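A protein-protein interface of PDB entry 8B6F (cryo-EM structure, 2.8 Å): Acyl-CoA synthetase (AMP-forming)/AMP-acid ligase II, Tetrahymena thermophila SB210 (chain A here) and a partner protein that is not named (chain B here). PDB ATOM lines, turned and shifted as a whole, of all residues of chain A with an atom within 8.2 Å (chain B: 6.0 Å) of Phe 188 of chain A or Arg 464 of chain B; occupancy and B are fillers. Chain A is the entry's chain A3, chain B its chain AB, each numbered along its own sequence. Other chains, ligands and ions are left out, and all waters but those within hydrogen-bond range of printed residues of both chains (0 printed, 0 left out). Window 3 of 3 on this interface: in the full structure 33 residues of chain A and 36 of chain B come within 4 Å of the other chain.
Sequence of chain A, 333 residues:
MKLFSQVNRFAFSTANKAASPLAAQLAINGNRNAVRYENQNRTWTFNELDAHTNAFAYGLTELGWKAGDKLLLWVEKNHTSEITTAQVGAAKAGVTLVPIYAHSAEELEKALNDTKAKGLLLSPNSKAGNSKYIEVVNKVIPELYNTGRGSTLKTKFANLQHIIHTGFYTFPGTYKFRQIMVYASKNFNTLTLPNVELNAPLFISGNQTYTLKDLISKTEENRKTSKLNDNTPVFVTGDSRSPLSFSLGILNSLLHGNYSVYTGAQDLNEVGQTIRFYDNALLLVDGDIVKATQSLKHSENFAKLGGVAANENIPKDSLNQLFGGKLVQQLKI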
ATOM      1  N   TYR A 183     -11.810  24.001  -0.362  1.00  0.00           N
ATOM      2  CA  TYR A 183     -12.320  24.505  -1.633  1.00  0.00           C
ATOM      3  C   TYR A 183     -13.840  24.577  -1.564  1.00  0.00           C
ATOM      4  O   TYR A 183     -14.519  23.547  -1.521  1.00  0.00           O
ATOM      5  CB  TYR A 183     -11.858  23.616  -2.783  1.00  0.00           C
ATOM      6  CG  TYR A 183     -10.366  23.664  -3.009  1.00  0.00           C
ATOM      7  CD1 TYR A 183      -9.504  22.897  -2.239  1.00  0.00           C
ATOM      8  CD2 TYR A 183      -9.821  24.485  -3.985  1.00  0.00           C
ATOM      9  CE1 TYR A 183      -8.139  22.942  -2.438  1.00  0.00           C
ATOM     10  CE2 TYR A 183      -8.458  24.537  -4.193  1.00  0.00           C
ATOM     11  CZ  TYR A 183      -7.622  23.764  -3.414  1.00  0.00           C
ATOM     12  OH  TYR A 183      -6.264  23.809  -3.617  1.00  0.00           O
ATOM     13  N   ALA A 184     -14.374  25.793  -1.560  1.00  0.00           N
ATOM     14  CA  ALA A 184     -15.810  25.987  -1.431  1.00  0.00           C
ATOM     15  C   ALA A 184     -16.549  25.419  -2.635  1.00  0.00           C
ATOM     16  O   ALA A 184     -16.066  25.459  -3.770  1.00  0.00           O
ATOM     17  CB  ALA A 184     -16.134  27.471  -1.274  1.00  0.00           C
ATOM     18  N   SER A 185     -17.738  24.884  -2.375  1.00  0.00           N
ATOM     19  CA  SER A 185     -18.578  24.347  -3.430  1.00  0.00           C
ATOM     20  C   SER A 185     -19.406  25.457  -4.068  1.00  0.00           C
ATOM     21  O   SER A 185     -19.586  26.540  -3.504  1.00  0.00           O
ATOM     22  CB  SER A 185     -19.506  23.264  -2.879  1.00  0.00           C
ATOM     23  OG  SER A 185     -18.772  22.252  -2.214  1.00  0.00           O
ATOM     24  N   LYS A 186     -19.912  25.175  -5.269  1.00  0.00           N
ATOM     25  CA  LYS A 186     -20.733  26.154  -5.972  1.00  0.00           C
ATOM     26  C   LYS A 186     -22.143  26.224  -5.396  1.00  0.00           C
ATOM     27  O   LYS A 186     -22.736  27.306  -5.336  1.00  0.00           O
ATOM     28  CB  LYS A 186     -20.785  25.822  -7.462  1.00  0.00           C
ATOM     29  CG  LYS A 186     -19.439  25.939  -8.163  1.00  0.00           C
ATOM     30  CD  LYS A 186     -19.561  25.702  -9.665  1.00  0.00           C
ATOM     31  CE  LYS A 186     -19.969  24.273  -9.992  1.00  0.00           C
ATOM     32  NZ  LYS A 186     -19.010  23.270  -9.448  1.00  0.00           N
ATOM     33  N   ASN A 187     -22.692  25.085  -4.962  1.00  0.00           N
ATOM     34  CA  ASN A 187     -24.055  25.025  -4.450  1.00  0.00           C
ATOM     35  C   ASN A 187     -24.142  24.412  -3.057  1.00  0.00           C
ATOM     36  O   ASN A 187     -25.253  24.164  -2.574  1.00  0.00           O
ATOM     37  CB  ASN A 187     -24.953  24.234  -5.409  1.00  0.00           C
ATOM     38  CG  ASN A 187     -25.063  24.883  -6.772  1.00  0.00           C
ATOM     39  OD1 ASN A 187     -24.931  26.099  -6.905  1.00  0.00           O
ATOM     40  ND2 ASN A 187     -25.308  24.073  -7.794  1.00  0.00           N
ATOM     41  N   PHE A 188     -23.012  24.153  -2.404  1.00  0.00           N
ATOM     42  CA  PHE A 188     -23.000  23.554  -1.074  1.00  0.00           C
ATOM     43  C   PHE A 188     -22.001  24.271  -0.177  1.00  0.00           C
ATOM     44  O   PHE A 188     -21.293  23.646   0.618  1.00  0.00           O
ATOM     45  CB  PHE A 188     -22.677  22.060  -1.146  1.00  0.00           C
ATOM     46  CG  PHE A 188     -23.659  21.266  -1.957  1.00  0.00           C
ATOM     47  CD1 PHE A 188     -24.792  20.733  -1.367  1.00  0.00           C
ATOM     48  CD2 PHE A 188     -23.446  21.045  -3.308  1.00  0.00           C
ATOM     49  CE1 PHE A 188     -25.697  19.999  -2.108  1.00  0.00           C
ATOM     50  CE2 PHE A 188     -24.347  20.311  -4.056  1.00  0.00           C
ATOM     51  CZ  PHE A 188     -25.474  19.788  -3.455  1.00  0.00           C
ATOM     52  N   ASN A 189     -21.930  25.594  -0.293  1.00  0.00           N
ATOM     53  CA  ASN A 189     -20.993  26.411   0.475  1.00  0.00           C
ATOM     54  C   ASN A 189     -21.782  27.245   1.479  1.00  0.00           C
ATOM     55  O   ASN A 189     -22.415  28.239   1.112  1.00  0.00           O
ATOM     56  CB  ASN A 189     -20.167  27.295  -0.454  1.00  0.00           C
ATOM     57  CG  ASN A 189     -19.302  28.281   0.301  1.00  0.00           C
ATOM     58  OD1 ASN A 189     -18.965  28.067   1.465  1.00  0.00           O
ATOM     59  ND2 ASN A 189     -18.936  29.373  -0.361  1.00  0.00           N
ATOM     60  N   THR A 190     -21.736  26.842   2.747  1.00  0.00           N
ATOM     61  CA  THR A 190     -22.397  27.580   3.814  1.00  0.00           C
ATOM     62  C   THR A 190     -21.493  28.610   4.477  1.00  0.00           C
ATOM     63  O   THR A 190     -21.967  29.362   5.335  1.00  0.00           O
ATOM     64  CB  THR A 190     -22.922  26.612   4.881  1.00  0.00           C
ATOM     65  OG1 THR A 190     -21.859  25.759   5.325  1.00  0.00           O
ATOM     66  CG2 THR A 190     -24.057  25.765   4.322  1.00  0.00           C
ATOM     67  N   LEU A 191     -20.218  28.663   4.108  1.00  0.00           N
ATOM     68  CA  LEU A 191     -19.306  29.639   4.682  1.00  0.00           C
ATOM     69  C   LEU A 191     -19.532  31.012   4.057  1.00  0.00           C
ATOM     70  O   LEU A 191     -20.148  31.150   2.997  1.00  0.00           O
ATOM     71  CB  LEU A 191     -17.855  29.203   4.477  1.00  0.00           C
ATOM     72  CG  LEU A 191     -17.468  27.844   5.066  1.00  0.00           C
ATOM     73  CD1 LEU A 191     -16.022  27.512   4.730  1.00  0.00           C
ATOM     74  CD2 LEU A 191     -17.686  27.815   6.570  1.00  0.00           C
ATOM     75  N   ASP B 398     -25.964   6.303  -5.664  1.00  0.00           N
ATOM     76  CA  ASP B 398     -25.992   7.488  -6.512  1.00  0.00           C
ATOM     77  C   ASP B 398     -25.174   8.635  -5.941  1.00  0.00           C
ATOM     78  O   ASP B 398     -24.617   9.431  -6.705  1.00  0.00           O
ATOM     79  CB  ASP B 398     -27.433   7.958  -6.729  1.00  0.00           C
ATOM     80  CG  ASP B 398     -28.271   6.942  -7.481  1.00  0.00           C
ATOM     81  OD1 ASP B 398     -27.765   5.831  -7.743  1.00  0.00           O
ATOM     82  OD2 ASP B 398     -29.432   7.258  -7.817  1.00  0.00           O
ATOM     83  N   VAL B 399     -25.112   8.754  -4.617  1.00  0.00           N
ATOM     84  CA  VAL B 399     -24.298   9.759  -3.944  1.00  0.00           C
ATOM     85  C   VAL B 399     -23.410   9.045  -2.936  1.00  0.00           C
ATOM     86  O   VAL B 399     -23.883   8.179  -2.191  1.00  0.00           O
ATOM     87  CB  VAL B 399     -25.162  10.827  -3.249  1.00  0.00           C
ATOM     88  CG1 VAL B 399     -24.282  11.878  -2.586  1.00  0.00           C
ATOM     89  CG2 VAL B 399     -26.107  11.474  -4.247  1.00  0.00           C
ATOM     90  N   LYS B 427     -22.186  10.719  -7.753  1.00  0.00           N
ATOM     91  CA  LYS B 427     -21.677  12.013  -7.320  1.00  0.00           C
ATOM     92  C   LYS B 427     -20.957  11.838  -5.990  1.00  0.00           C
ATOM     93  O   LYS B 427     -21.511  11.254  -5.053  1.00  0.00           O
ATOM     94  CB  LYS B 427     -22.812  13.029  -7.184  1.00  0.00           C
ATOM     95  CG  LYS B 427     -23.657  13.188  -8.441  1.00  0.00           C
ATOM     96  CD  LYS B 427     -22.825  13.676  -9.618  1.00  0.00           C
ATOM     97  CE  LYS B 427     -23.681  13.850 -10.863  1.00  0.00           C
ATOM     98  NZ  LYS B 427     -22.874  14.317 -12.024  1.00  0.00           N
ATOM     99  N   PHE B 429     -18.909  13.396  -2.714  1.00  0.00           N
ATOM    100  CA  PHE B 429     -18.689  14.521  -1.820  1.00  0.00           C
ATOM    101  C   PHE B 429     -17.659  14.125  -0.771  1.00  0.00           C
ATOM    102  O   PHE B 429     -17.540  12.951  -0.412  1.00  0.00           O
ATOM    103  CB  PHE B 429     -19.990  14.956  -1.141  1.00  0.00           C
ATOM    104  CG  PHE B 429     -21.033  15.449  -2.099  1.00  0.00           C
ATOM    105  CD1 PHE B 429     -21.717  14.564  -2.916  1.00  0.00           C
ATOM    106  CD2 PHE B 429     -21.346  16.795  -2.165  1.00  0.00           C
ATOM    107  CE1 PHE B 429     -22.682  15.017  -3.794  1.00  0.00           C
ATOM    108  CE2 PHE B 429     -22.309  17.255  -3.038  1.00  0.00           C
ATOM    109  CZ  PHE B 429     -22.979  16.364  -3.854  1.00  0.00           C
ATOM    110  N   VAL B 442     -16.895  17.036  -4.714  1.00  0.00           N
ATOM    111  CA  VAL B 442     -17.371  18.278  -4.120  1.00  0.00           C
ATOM    112  C   VAL B 442     -16.863  18.334  -2.687  1.00  0.00           C
ATOM    113  O   VAL B 442     -17.240  17.498  -1.855  1.00  0.00           O
ATOM    114  CB  VAL B 442     -18.904  18.371  -4.172  1.00  0.00           C
ATOM    115  CG1 VAL B 442     -19.389  19.651  -3.509  1.00  0.00           C
ATOM    116  CG2 VAL B 442     -19.390  18.291  -5.608  1.00  0.00           C
ATOM    117  N   HIS B 443     -16.010  19.310  -2.394  1.00  0.00           N
ATOM    118  CA  HIS B 443     -15.378  19.423  -1.081  1.00  0.00           C
ATOM    119  C   HIS B 443     -16.257  20.301  -0.198  1.00  0.00           C
ATOM    120  O   HIS B 443     -16.261  21.526  -0.329  1.00  0.00           O
ATOM    121  CB  HIS B 443     -13.969  19.987  -1.209  1.00  0.00           C
ATOM    122  CG  HIS B 443     -13.176  19.921   0.059  1.00  0.00           C
ATOM    123  ND1 HIS B 443     -12.104  20.749   0.308  1.00  0.00           N
ATOM    124  CD2 HIS B 443     -13.296  19.123   1.145  1.00  0.00           C
ATOM    125  CE1 HIS B 443     -11.598  20.466   1.495  1.00  0.00           C
ATOM    126  NE2 HIS B 443     -12.303  19.483   2.024  1.00  0.00           N
ATOM    127  N   LEU B 444     -17.005  19.672   0.711  1.00  0.00           N
ATOM    128  CA  LEU B 444     -17.897  20.426   1.585  1.00  0.00           C
ATOM    129  C   LEU B 444     -17.129  21.158   2.678  1.00  0.00           C
ATOM    130  O   LEU B 444     -17.482  22.285   3.039  1.00  0.00           O
ATOM    131  CB  LEU B 444     -18.937  19.490   2.199  1.00  0.00           C
ATOM    132  CG  LEU B 444     -19.832  18.745   1.205  1.00  0.00           C
ATOM    133  CD1 LEU B 444     -20.754  17.783   1.933  1.00  0.00           C
ATOM    134  CD2 LEU B 444     -20.639  19.717   0.359  1.00  0.00           C
ATOM    135  N   HIS B 459     -27.923  22.220   6.764  1.00  0.00           N
ATOM    136  CA  HIS B 459     -27.024  22.127   5.623  1.00  0.00           C
ATOM    137  C   HIS B 459     -27.783  21.613   4.401  1.00  0.00           C
ATOM    138  O   HIS B 459     -28.558  20.660   4.510  1.00  0.00           O
ATOM    139  CB  HIS B 459     -25.859  21.194   5.941  1.00  0.00           C
ATOM    140  CG  HIS B 459     -24.666  21.394   5.059  1.00  0.00           C
ATOM    141  ND1 HIS B 459     -23.993  22.595   4.975  1.00  0.00           N
ATOM    142  CD2 HIS B 459     -24.021  20.544   4.225  1.00  0.00           C
ATOM    143  CE1 HIS B 459     -22.989  22.477   4.125  1.00  0.00           C
ATOM    144  NE2 HIS B 459     -22.982  21.242   3.657  1.00  0.00           N
ATOM    145  N   PRO B 460     -27.581  22.215   3.226  1.00  0.00           N
ATOM    146  CA  PRO B 460     -28.304  21.738   2.036  1.00  0.00           C
ATOM    147  C   PRO B 460     -27.979  20.307   1.658  1.00  0.00           C
ATOM    148  O   PRO B 460     -28.767  19.678   0.942  1.00  0.00           O
ATOM    149  CB  PRO B 460     -27.869  22.719   0.939  1.00  0.00           C
ATOM    150  CG  PRO B 460     -26.578  23.275   1.413  1.00  0.00           C
ATOM    151  CD  PRO B 460     -26.682  23.337   2.904  1.00  0.00           C
ATOM    152  N   PHE B 461     -26.847  19.765   2.112  1.00  0.00           N
ATOM    153  CA  PHE B 461     -26.526  18.379   1.800  1.00  0.00           C
ATOM    154  C   PHE B 461     -27.506  17.405   2.438  1.00  0.00           C
ATOM    155  O   PHE B 461     -27.652  16.282   1.944  1.00  0.00           O
ATOM    156  CB  PHE B 461     -25.104  18.043   2.247  1.00  0.00           C
ATOM    157  CG  PHE B 461     -24.600  16.749   1.692  1.00  0.00           C
ATOM    158  CD1 PHE B 461     -24.136  16.675   0.392  1.00  0.00           C
ATOM    159  CD2 PHE B 461     -24.606  15.602   2.463  1.00  0.00           C
ATOM    160  CE1 PHE B 461     -23.679  15.482  -0.126  1.00  0.00           C
ATOM    161  CE2 PHE B 461     -24.152  14.407   1.949  1.00  0.00           C
ATOM    162  CZ  PHE B 461     -23.686  14.346   0.653  1.00  0.00           C
ATOM    163  N   ALA B 462     -28.181  17.803   3.518  1.00  0.00           N
ATOM    164  CA  ALA B 462     -29.232  16.961   4.077  1.00  0.00           C
ATOM    165  C   ALA B 462     -30.368  16.791   3.078  1.00  0.00           C
ATOM    166  O   ALA B 462     -30.841  15.674   2.838  1.00  0.00           O
ATOM    167  CB  ALA B 462     -29.746  17.562   5.386  1.00  0.00           C
ATOM    168  N   GLU B 463     -30.819  17.896   2.483  1.00  0.00           N
ATOM    169  CA  GLU B 463     -31.834  17.808   1.439  1.00  0.00           C
ATOM    170  C   GLU B 463     -31.308  17.033   0.238  1.00  0.00           C
ATOM    171  O   GLU B 463     -32.055  16.284  -0.403  1.00  0.00           O
ATOM    172  CB  GLU B 463     -32.278  19.210   1.021  1.00  0.00           C
ATOM    173  CG  GLU B 463     -32.834  20.046   2.162  1.00  0.00           C
ATOM    174  CD  GLU B 463     -33.179  21.458   1.732  1.00  0.00           C
ATOM    175  OE1 GLU B 463     -32.997  21.777   0.539  1.00  0.00           O
ATOM    176  OE2 GLU B 463     -33.633  22.249   2.586  1.00  0.00           O
ATOM    177  N   ARG B 464     -30.025  17.205  -0.082  1.00  0.00           N
ATOM    178  CA  ARG B 464     -29.427  16.467  -1.191  1.00  0.00           C
ATOM    179  C   ARG B 464     -29.498  14.964  -0.945  1.00  0.00           C
ATOM    180  O   ARG B 464     -29.872  14.193  -1.835  1.00  0.00           O
ATOM    181  CB  ARG B 464     -27.979  16.915  -1.390  1.00  0.00           C
ATOM    182  CG  ARG B 464     -27.270  16.254  -2.564  1.00  0.00           C
ATOM    183  CD  ARG B 464     -27.938  16.611  -3.883  1.00  0.00           C
ATOM    184  NE  ARG B 464     -27.201  16.097  -5.032  1.00  0.00           N
ATOM    185  CZ  ARG B 464     -27.349  14.880  -5.539  1.00  0.00           C
ATOM    186  NH1 ARG B 464     -28.199  14.011  -5.019  1.00  0.00           N
ATOM    187  NH2 ARG B 464     -26.624  14.527  -6.596  1.00  0.00           N
ATOM    188  N   LEU B 465     -29.134  14.528   0.263  1.00  0.00           N
ATOM    189  CA  LEU B 465     -29.222  13.109   0.590  1.00  0.00           C
ATOM    190  C   LEU B 465     -30.663  12.621   0.544  1.00  0.00           C
ATOM    191  O   LEU B 465     -30.942  11.531   0.033  1.00  0.00           O
ATOM    192  CB  LEU B 465     -28.619  12.847   1.969  1.00  0.00           C
ATOM    193  CG  LEU B 465     -27.101  12.969   2.100  1.00  0.00           C
ATOM    194  CD1 LEU B 465     -26.685  12.789   3.550  1.00  0.00           C
ATOM    195  CD2 LEU B 465     -26.389  11.957   1.214  1.00  0.00           C
ATOM    196  N   LYS B 466     -31.596  13.412   1.079  1.00  0.00           N
ATOM    197  CA  LYS B 466     -32.997  13.010   1.054  1.00  0.00           C
ATOM    198  C   LYS B 466     -33.486  12.826  -0.376  1.00  0.00           C
ATOM    199  O   LYS B 466     -34.195  11.860  -0.680  1.00  0.00           O
ATOM    200  CB  LYS B 466     -33.849  14.046   1.789  1.00  0.00           C
ATOM    201  CG  LYS B 466     -33.600  14.095   3.291  1.00  0.00           C
ATOM    202  CD  LYS B 466     -34.351  15.246   3.946  1.00  0.00           C
ATOM    203  CE  LYS B 466     -34.054  15.317   5.437  1.00  0.00           C
ATOM    204  NZ  LYS B 466     -34.751  16.458   6.096  1.00  0.00           N
ATOM    205  N   LYS B 467     -33.113  13.743  -1.271  1.00  0.00           N
ATOM    206  CA  LYS B 467     -33.490  13.599  -2.672  1.00  0.00           C
ATOM    207  C   LYS B 467     -32.841  12.368  -3.290  1.00  0.00           C
ATOM    208  O   LYS B 467     -33.492  11.617  -4.026  1.00  0.00           O
ATOM    209  CB  LYS B 467     -33.100  14.856  -3.450  1.00  0.00           C
ATOM    210  CG  LYS B 467     -33.575  14.857  -4.899  1.00  0.00           C
ATOM    211  CD  LYS B 467     -33.040  16.054  -5.673  1.00  0.00           C
ATOM    212  CE  LYS B 467     -31.549  15.921  -5.951  1.00  0.00           C
ATOM    213  NZ  LYS B 467     -31.039  17.031  -6.807  1.00  0.00           N
ATOM    214  N   ALA B 468     -31.564  12.142  -3.000  1.00  0.00           N
ATOM    215  CA  ALA B 468     -30.840  11.038  -3.610  1.00  0.00           C
ATOM    216  C   ALA B 468     -31.380   9.698  -3.125  1.00  0.00           C
ATOM    217  O   ALA B 468     -31.863   9.564  -1.998  1.00  0.00           O
ATOM    218  CB  ALA B 468     -29.349  11.137  -3.292  1.00  0.00           C
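Of the 9 printed residues of chain A, 4 touch a printed residue of chain B.
Hydrophobic or aromatic side chains of chain A that line the printed part of chain B: Phe 188.
Hydrophobic or aromatic side chains of chain B that line the printed part of chain A: Phe 429, Val 442, His 443, Leu 444, His 459 and Pro 460.
Among the printed residues, 8 pairs touch across the chains.
A ring nitrogen (ND1) of His 443 of chain B is in hydrogen-bond range of the backbone NH of Tyr 183 of chain A, at 3.3 Å.
OG of Ser 185 of chain A is in hydrogen-bond range of O of His 443 of chain B, 3.2 Å away.
Phe 188 of chain A touches just these residues of chain B: Phe 429 (3.8 Å), Leu 444 (3.5 Å) and Arg 464 (3.9 Å).
Of chain A, only Phe 188 comes within 4 Å of Arg 464 of chain B.
Of the printed residues of chain B, Tyr 183 of chain A touches His 443.
Of the printed residues of chain A, Val 442 of chain B touches Ser 185.
Printed residues of chain A within 4 Å of His 443 of chain B: Tyr 183 (2.9 Å) and Ser 185 (3.2 Å).
Of the printed residues of chain A, Pro 460 of chain B touches Thr 190.
The nearest residue of chain B that does not touch Phe 188 of chain A is His 459 of chain B (4.1 Å).
The nearest residue of chain A that does not touch Arg 464 of chain B is Asn 187 of chain A (7.8 Å).
Among the printed residues, merely in contact across the chains: Ser 185 of chain A with Val 442 of chain B (3.0 Å), Thr 190 of chain A with His 459 of chain B (3.2 Å), Phe 188 of chain A with Leu 444 of chain B (3.5 Å), Phe 188 of chain A with Phe 429 of chain B (3.8 Å), Thr 190 of chain A with Pro 460 of chain B (3.8 Å) and Phe 188 of chain A with Arg 464 of chain B (3.9 Å).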
